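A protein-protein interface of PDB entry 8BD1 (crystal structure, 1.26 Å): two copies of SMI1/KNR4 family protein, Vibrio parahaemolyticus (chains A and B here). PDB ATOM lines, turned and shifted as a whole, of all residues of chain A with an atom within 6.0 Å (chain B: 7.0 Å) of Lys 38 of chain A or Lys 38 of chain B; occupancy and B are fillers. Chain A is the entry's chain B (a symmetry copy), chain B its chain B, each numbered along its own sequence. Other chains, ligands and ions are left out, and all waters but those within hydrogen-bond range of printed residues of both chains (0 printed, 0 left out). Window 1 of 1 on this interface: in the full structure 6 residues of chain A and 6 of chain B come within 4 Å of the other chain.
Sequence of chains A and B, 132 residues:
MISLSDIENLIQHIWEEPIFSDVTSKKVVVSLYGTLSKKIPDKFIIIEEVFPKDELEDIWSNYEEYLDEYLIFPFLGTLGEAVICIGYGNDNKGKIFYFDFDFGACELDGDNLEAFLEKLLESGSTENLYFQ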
ATOM      1  N   TYR A  33      -8.874   7.097 -25.104  1.00  0.00           N
ATOM      2  CA  TYR A  33      -7.956   8.171 -25.465  1.00  0.00           C
ATOM      3  C   TYR A  33      -6.659   7.962 -24.690  1.00  0.00           C
ATOM      4  O   TYR A  33      -6.597   8.227 -23.485  1.00  0.00           O
ATOM      5  CB  TYR A  33      -8.606   9.519 -25.153  1.00  0.00           C
ATOM      6  CG  TYR A  33      -9.856   9.760 -25.972  1.00  0.00           C
ATOM      7  CD1 TYR A  33      -9.767  10.012 -27.338  1.00  0.00           C
ATOM      8  CD2 TYR A  33     -11.119   9.707 -25.400  1.00  0.00           C
ATOM      9  CE1 TYR A  33     -10.892  10.220 -28.099  1.00  0.00           C
ATOM     10  CE2 TYR A  33     -12.260   9.922 -26.161  1.00  0.00           C
ATOM     11  CZ  TYR A  33     -12.136  10.173 -27.508  1.00  0.00           C
ATOM     12  OH  TYR A  33     -13.266  10.396 -28.268  1.00  0.00           O
ATOM     13  N   GLY A  34      -5.616   7.499 -25.386  1.00  0.00           N
ATOM     14  CA  GLY A  34      -4.419   7.043 -24.693  1.00  0.00           C
ATOM     15  C   GLY A  34      -3.734   8.139 -23.902  1.00  0.00           C
ATOM     16  O   GLY A  34      -3.441   7.977 -22.715  1.00  0.00           O
ATOM     17  N   THR A  35      -3.483   9.278 -24.543  1.00  0.00           N
ATOM     18  CA  THR A  35      -2.794  10.360 -23.853  1.00  0.00           C
ATOM     19  C   THR A  35      -3.623  10.874 -22.686  1.00  0.00           C
ATOM     20  O   THR A  35      -3.095  11.076 -21.589  1.00  0.00           O
ATOM     21  CB  THR A  35      -2.454  11.487 -24.829  1.00  0.00           C
ATOM     22  OG1 THR A  35      -1.646  10.956 -25.888  1.00  0.00           O
ATOM     23  CG2 THR A  35      -1.679  12.574 -24.116  1.00  0.00           C
ATOM     24  N   LEU A  36      -4.930  11.064 -22.895  1.00  0.00           N
ATOM     25  CA  LEU A  36      -5.781  11.520 -21.802  1.00  0.00           C
ATOM     26  C   LEU A  36      -5.745  10.541 -20.637  1.00  0.00           C
ATOM     27  O   LEU A  36      -5.684  10.953 -19.473  1.00  0.00           O
ATOM     28  CB  LEU A  36      -7.214  11.706 -22.287  1.00  0.00           C
ATOM     29  CG  LEU A  36      -8.169  12.279 -21.233  1.00  0.00           C
ATOM     30  CD1 LEU A  36      -7.710  13.671 -20.792  1.00  0.00           C
ATOM     31  CD2 LEU A  36      -9.603  12.323 -21.777  1.00  0.00           C
ATOM     32  N   SER A  37      -5.770   9.238 -20.934  1.00  0.00           N
ATOM     33  CA  SER A  37      -5.778   8.247 -19.865  1.00  0.00           C
ATOM     34  C   SER A  37      -4.500   8.289 -19.032  1.00  0.00           C
ATOM     35  O   SER A  37      -4.522   7.908 -17.853  1.00  0.00           O
ATOM     36  CB  SER A  37      -6.057   6.853 -20.417  1.00  0.00           C
ATOM     37  OG  SER A  37      -4.964   6.364 -21.150  1.00  0.00           O
ATOM     38  N   LYS A  38      -3.382   8.734 -19.614  1.00  0.00           N
ATOM     39  CA  LYS A  38      -2.153   8.915 -18.846  1.00  0.00           C
ATOM     40  C   LYS A  38      -2.115  10.235 -18.093  1.00  0.00           C
ATOM     41  O   LYS A  38      -1.315  10.384 -17.160  1.00  0.00           O
ATOM     42  CB  LYS A  38      -0.943   8.848 -19.772  1.00  0.00           C
ATOM     43  CG  LYS A  38      -0.763   7.490 -20.389  1.00  0.00           C
ATOM     44  CD  LYS A  38       0.498   7.412 -21.213  1.00  0.00           C
ATOM     45  CE  LYS A  38       0.377   8.241 -22.474  1.00  0.00           C
ATOM     46  NZ  LYS A  38       1.652   8.201 -23.253  1.00  0.00           N
ATOM     47  N   LYS A  39      -2.933  11.197 -18.478  1.00  0.00           N
ATOM     48  CA  LYS A  39      -2.874  12.519 -17.876  1.00  0.00           C
ATOM     49  C   LYS A  39      -3.815  12.687 -16.691  1.00  0.00           C
ATOM     50  O   LYS A  39      -3.508  13.452 -15.769  1.00  0.00           O
ATOM     51  CB  LYS A  39      -3.200  13.571 -18.935  1.00  0.00           C
ATOM     52  CG  LYS A  39      -3.060  15.003 -18.469  1.00  0.00           C
ATOM     53  CD  LYS A  39      -3.160  15.980 -19.634  1.00  0.00           C
ATOM     54  CE  LYS A  39      -2.141  15.641 -20.711  1.00  0.00           C
ATOM     55  NZ  LYS A  39      -1.707  16.856 -21.470  1.00  0.00           N
ATOM     56  N   ILE A  40      -4.966  12.024 -16.693  1.00  0.00           N
ATOM     57  CA  ILE A  40      -5.948  12.239 -15.631  1.00  0.00           C
ATOM     58  C   ILE A  40      -6.320  10.901 -15.023  1.00  0.00           C
ATOM     59  O   ILE A  40      -6.186   9.852 -15.666  1.00  0.00           O
ATOM     60  CB  ILE A  40      -7.202  12.989 -16.144  1.00  0.00           C
ATOM     61  CG1 ILE A  40      -8.030  12.127 -17.107  1.00  0.00           C
ATOM     62  CG2 ILE A  40      -6.817  14.320 -16.754  1.00  0.00           C
ATOM     63  CD1 ILE A  40      -9.379  12.750 -17.451  1.00  0.00           C
ATOM     64  N   VAL B  30       7.054   3.708 -13.251  1.00  0.00           N
ATOM     65  CA  VAL B  30       6.141   3.217 -14.285  1.00  0.00           C
ATOM     66  C   VAL B  30       5.784   4.324 -15.269  1.00  0.00           C
ATOM     67  O   VAL B  30       5.629   4.077 -16.473  1.00  0.00           O
ATOM     68  CB  VAL B  30       4.891   2.580 -13.649  1.00  0.00           C
ATOM     69  CG1 VAL B  30       3.857   2.243 -14.719  1.00  0.00           C
ATOM     70  CG2 VAL B  30       5.270   1.342 -12.845  1.00  0.00           C
ATOM     71  N   SER B  31       5.671   5.566 -14.784  1.00  0.00           N
ATOM     72  CA  SER B  31       5.260   6.662 -15.658  1.00  0.00           C
ATOM     73  C   SER B  31       6.277   6.978 -16.749  1.00  0.00           C
ATOM     74  O   SER B  31       5.933   7.702 -17.690  1.00  0.00           O
ATOM     75  CB  SER B  31       4.925   7.921 -14.852  1.00  0.00           C
ATOM     76  OG  SER B  31       5.971   8.243 -13.957  1.00  0.00           O
ATOM     77  N   TYR B  33       7.110   4.812 -18.790  1.00  0.00           N
ATOM     78  CA  TYR B  33       6.749   3.829 -19.805  1.00  0.00           C
ATOM     79  C   TYR B  33       5.268   4.007 -20.127  1.00  0.00           C
ATOM     80  O   TYR B  33       4.402   3.611 -19.342  1.00  0.00           O
ATOM     81  CB  TYR B  33       7.062   2.426 -19.285  1.00  0.00           C
ATOM     82  CG  TYR B  33       8.541   2.222 -19.030  1.00  0.00           C
ATOM     83  CD1 TYR B  33       9.434   2.130 -20.093  1.00  0.00           C
ATOM     84  CD2 TYR B  33       9.051   2.152 -17.742  1.00  0.00           C
ATOM     85  CE1 TYR B  33      10.781   1.958 -19.879  1.00  0.00           C
ATOM     86  CE2 TYR B  33      10.409   1.972 -17.518  1.00  0.00           C
ATOM     87  CZ  TYR B  33      11.265   1.881 -18.592  1.00  0.00           C
ATOM     88  OH  TYR B  33      12.615   1.694 -18.376  1.00  0.00           O
ATOM     89  N   GLY B  34       4.979   4.593 -21.294  1.00  0.00           N
ATOM     90  CA  GLY B  34       3.616   5.023 -21.577  1.00  0.00           C
ATOM     91  C   GLY B  34       2.625   3.876 -21.612  1.00  0.00           C
ATOM     92  O   GLY B  34       1.585   3.916 -20.951  1.00  0.00           O
ATOM     93  N   THR B  35       2.941   2.830 -22.371  1.00  0.00           N
ATOM     94  CA  THR B  35       2.016   1.710 -22.479  1.00  0.00           C
ATOM     95  C   THR B  35       1.828   1.030 -21.131  1.00  0.00           C
ATOM     96  O   THR B  35       0.698   0.729 -20.738  1.00  0.00           O
ATOM     97  CB  THR B  35       2.498   0.717 -23.537  1.00  0.00           C
ATOM     98  OG1 THR B  35       2.626   1.401 -24.791  1.00  0.00           O
ATOM     99  CG2 THR B  35       1.497  -0.408 -23.688  1.00  0.00           C
ATOM    100  N   LEU B  36       2.922   0.805 -20.396  1.00  0.00           N
ATOM    101  CA  LEU B  36       2.799   0.189 -19.080  1.00  0.00           C
ATOM    102  C   LEU B  36       1.922   1.031 -18.165  1.00  0.00           C
ATOM    103  O   LEU B  36       1.091   0.494 -17.424  1.00  0.00           O
ATOM    104  CB  LEU B  36       4.176  -0.005 -18.454  1.00  0.00           C
ATOM    105  CG  LEU B  36       4.159  -0.737 -17.106  1.00  0.00           C
ATOM    106  CD1 LEU B  36       3.587  -2.147 -17.267  1.00  0.00           C
ATOM    107  CD2 LEU B  36       5.570  -0.785 -16.506  1.00  0.00           C
ATOM    108  N   SER B  37       2.085   2.357 -18.211  1.00  0.00           N
ATOM    109  CA  SER B  37       1.306   3.219 -17.332  1.00  0.00           C
ATOM    110  C   SER B  37      -0.189   3.142 -17.628  1.00  0.00           C
ATOM    111  O   SER B  37      -1.007   3.386 -16.730  1.00  0.00           O
ATOM    112  CB  SER B  37       1.826   4.652 -17.375  1.00  0.00           C
ATOM    113  OG  SER B  37       1.524   5.271 -18.598  1.00  0.00           O
ATOM    114  N   LYS B  38      -0.570   2.818 -18.868  1.00  0.00           N
ATOM    115  CA  LYS B  38      -1.979   2.607 -19.192  1.00  0.00           C
ATOM    116  C   LYS B  38      -2.467   1.213 -18.831  1.00  0.00           C
ATOM    117  O   LYS B  38      -3.683   0.997 -18.737  1.00  0.00           O
ATOM    118  CB  LYS B  38      -2.212   2.834 -20.682  1.00  0.00           C
ATOM    119  CG  LYS B  38      -1.976   4.260 -21.092  1.00  0.00           C
ATOM    120  CD  LYS B  38      -2.317   4.488 -22.545  1.00  0.00           C
ATOM    121  CE  LYS B  38      -1.318   3.802 -23.453  1.00  0.00           C
ATOM    122  NZ  LYS B  38      -1.699   3.988 -24.886  1.00  0.00           N
ATOM    123  N   LYS B  39      -1.568   0.265 -18.647  1.00  0.00           N
ATOM    124  CA  LYS B  39      -1.967  -1.113 -18.409  1.00  0.00           C
ATOM    125  C   LYS B  39      -2.102  -1.456 -16.932  1.00  0.00           C
ATOM    126  O   LYS B  39      -2.927  -2.306 -16.574  1.00  0.00           O
ATOM    127  CB  LYS B  39      -0.950  -2.052 -19.057  1.00  0.00           C
ATOM    128  CG  LYS B  39      -1.308  -3.520 -18.984  1.00  0.00           C
ATOM    129  CD  LYS B  39      -0.385  -4.362 -19.854  1.00  0.00           C
ATOM    130  CE  LYS B  39      -0.388  -3.858 -21.289  1.00  0.00           C
ATOM    131  NZ  LYS B  39      -0.119  -4.957 -22.268  1.00  0.00           N
ATOM    132  N   ILE B  40      -1.303  -0.851 -16.061  1.00  0.00           N
ATOM    133  CA  ILE B  40      -1.321  -1.229 -14.649  1.00  0.00           C
ATOM    134  C   ILE B  40      -1.536   0.013 -13.807  1.00  0.00           C
ATOM    135  O   ILE B  40      -1.235   1.133 -14.239  1.00  0.00           O
ATOM    136  CB  ILE B  40      -0.029  -1.973 -14.231  1.00  0.00           C
ATOM    137  CG1 ILE B  40       1.195  -1.047 -14.246  1.00  0.00           C
ATOM    138  CG2 ILE B  40       0.178  -3.207 -15.082  1.00  0.00           C
ATOM    139  CD1 ILE B  40       2.433  -1.688 -13.627  1.00  0.00           C
ATOM    140  N   PRO B  41      -2.034  -0.151 -12.578  1.00  0.00           N
ATOM    141  CA  PRO B  41      -2.233   1.009 -11.701  1.00  0.00           C
ATOM    142  C   PRO B  41      -0.988   1.432 -10.943  1.00  0.00           C
ATOM    143  O   PRO B  41      -0.954   2.563 -10.442  1.00  0.00           O
ATOM    144  CB  PRO B  41      -3.308   0.516 -10.723  1.00  0.00           C
ATOM    145  CG  PRO B  41      -3.074  -0.944 -10.636  1.00  0.00           C
ATOM    146  CD  PRO B  41      -2.649  -1.371 -12.026  1.00  0.00           C
ATOM    147  N   LYS B  43       2.369   2.948  -9.597  1.00  0.00           N
ATOM    148  CA  LYS B  43       3.242   4.047  -9.986  1.00  0.00           C
ATOM    149  C   LYS B  43       4.707   3.639  -9.985  1.00  0.00           C
ATOM    150  O   LYS B  43       5.502   4.194 -10.749  1.00  0.00           O
ATOM    151  CB  LYS B  43       3.069   5.246  -9.044  1.00  0.00           C
ATOM    152  CG  LYS B  43       1.697   5.914  -9.111  1.00  0.00           C
ATOM    153  CD  LYS B  43       1.374   6.407 -10.522  1.00  0.00           C
ATOM    154  CE  LYS B  43      -0.015   7.024 -10.595  1.00  0.00           C
ATOM    155  NZ  LYS B  43      -0.378   7.367 -12.000  1.00  0.00           N
ATOM    156  N   PHE B 131       4.100  15.276 -13.342  1.00  0.00           N
ATOM    157  CA  PHE B 131       3.126  14.781 -14.309  1.00  0.00           C
ATOM    158  C   PHE B 131       3.777  14.777 -15.696  1.00  0.00           C
ATOM    159  O   PHE B 131       3.816  13.748 -16.371  1.00  0.00           O
ATOM    160  CB  PHE B 131       1.877  15.668 -14.347  1.00  0.00           C
ATOM    161  CG  PHE B 131       1.143  15.796 -13.024  1.00  0.00           C
ATOM    162  CD1 PHE B 131       1.241  14.818 -12.040  1.00  0.00           C
ATOM    163  CD2 PHE B 131       0.329  16.889 -12.791  1.00  0.00           C
ATOM    164  CE1 PHE B 131       0.542  14.943 -10.839  1.00  0.00           C
ATOM    165  CE2 PHE B 131      -0.363  17.028 -11.599  1.00  0.00           C
ATOM    166  CZ  PHE B 131      -0.250  16.054 -10.615  1.00  0.00           C
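Printed residues of chain B within 4 Å of Lys 38 of chain A: Gly 34 (3.7 Å), Ser 37 (3.5 Å) and Lys 38 (3.5 Å).
Lys 38 of chain B touches just these residues of chain A: Gly 34, Ser 37 and Lys 38.
Printed residues of chain B within 4 Å of Gly 34 of chain A: Lys 38.
Of the printed residues of chain A, Gly 34 of chain B touches Lys 38.
The nearest residue of chain B that does not touch Lys 38 of chain A is Thr 35 of chain B (5.3 Å).
Of the 13 printed residues of chain B, 3 touch a printed residue of chain A.
Among the printed residues, 5 pairs touch across the chains.
Among the printed residues, no Asp or Glu carboxylate lies within 4 Å of a Lys or Arg side-chain nitrogen of the other chain.
Gly 34 of chain A touches Lys 38 of chain B, and with the chains exchanged Lys 38 of chain A touches Gly 34 of chain B.
Ser 37 of chain A touches Lys 38 of chain B, and with the chains exchanged Lys 38 of chain A touches Ser 37 of chain B.
Lys 38 of chain B touches its own counterpart, Lys 38 of chain A.
8 positions are printed for both chains.
O of Tyr 33 of chain B sits close to OG of Ser 37 of chain B, 3.4 Å away.
O of Tyr 33 of chain A lies close to OG of Ser 37 of chain A, 3.4 Å away.
O of Gly 34 of chain B is in hydrogen-bond range of OG of Ser 37 of chain B.
OG of Ser 37 of chain A is in hydrogen-bond range of O of Gly 34 of chain A (2.7 Å).
Among the printed residues, pairs that only touch across the chains: Gly 34 of chain A with Lys 38 of chain B, Ser 37 of chain A with Lys 38 of chain B, Lys 38 of chain A with Gly 34 of chain B, Lys 38 of chain A with Ser 37 of chain B and Lys 38 of chain A with Lys 38 of chain B.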
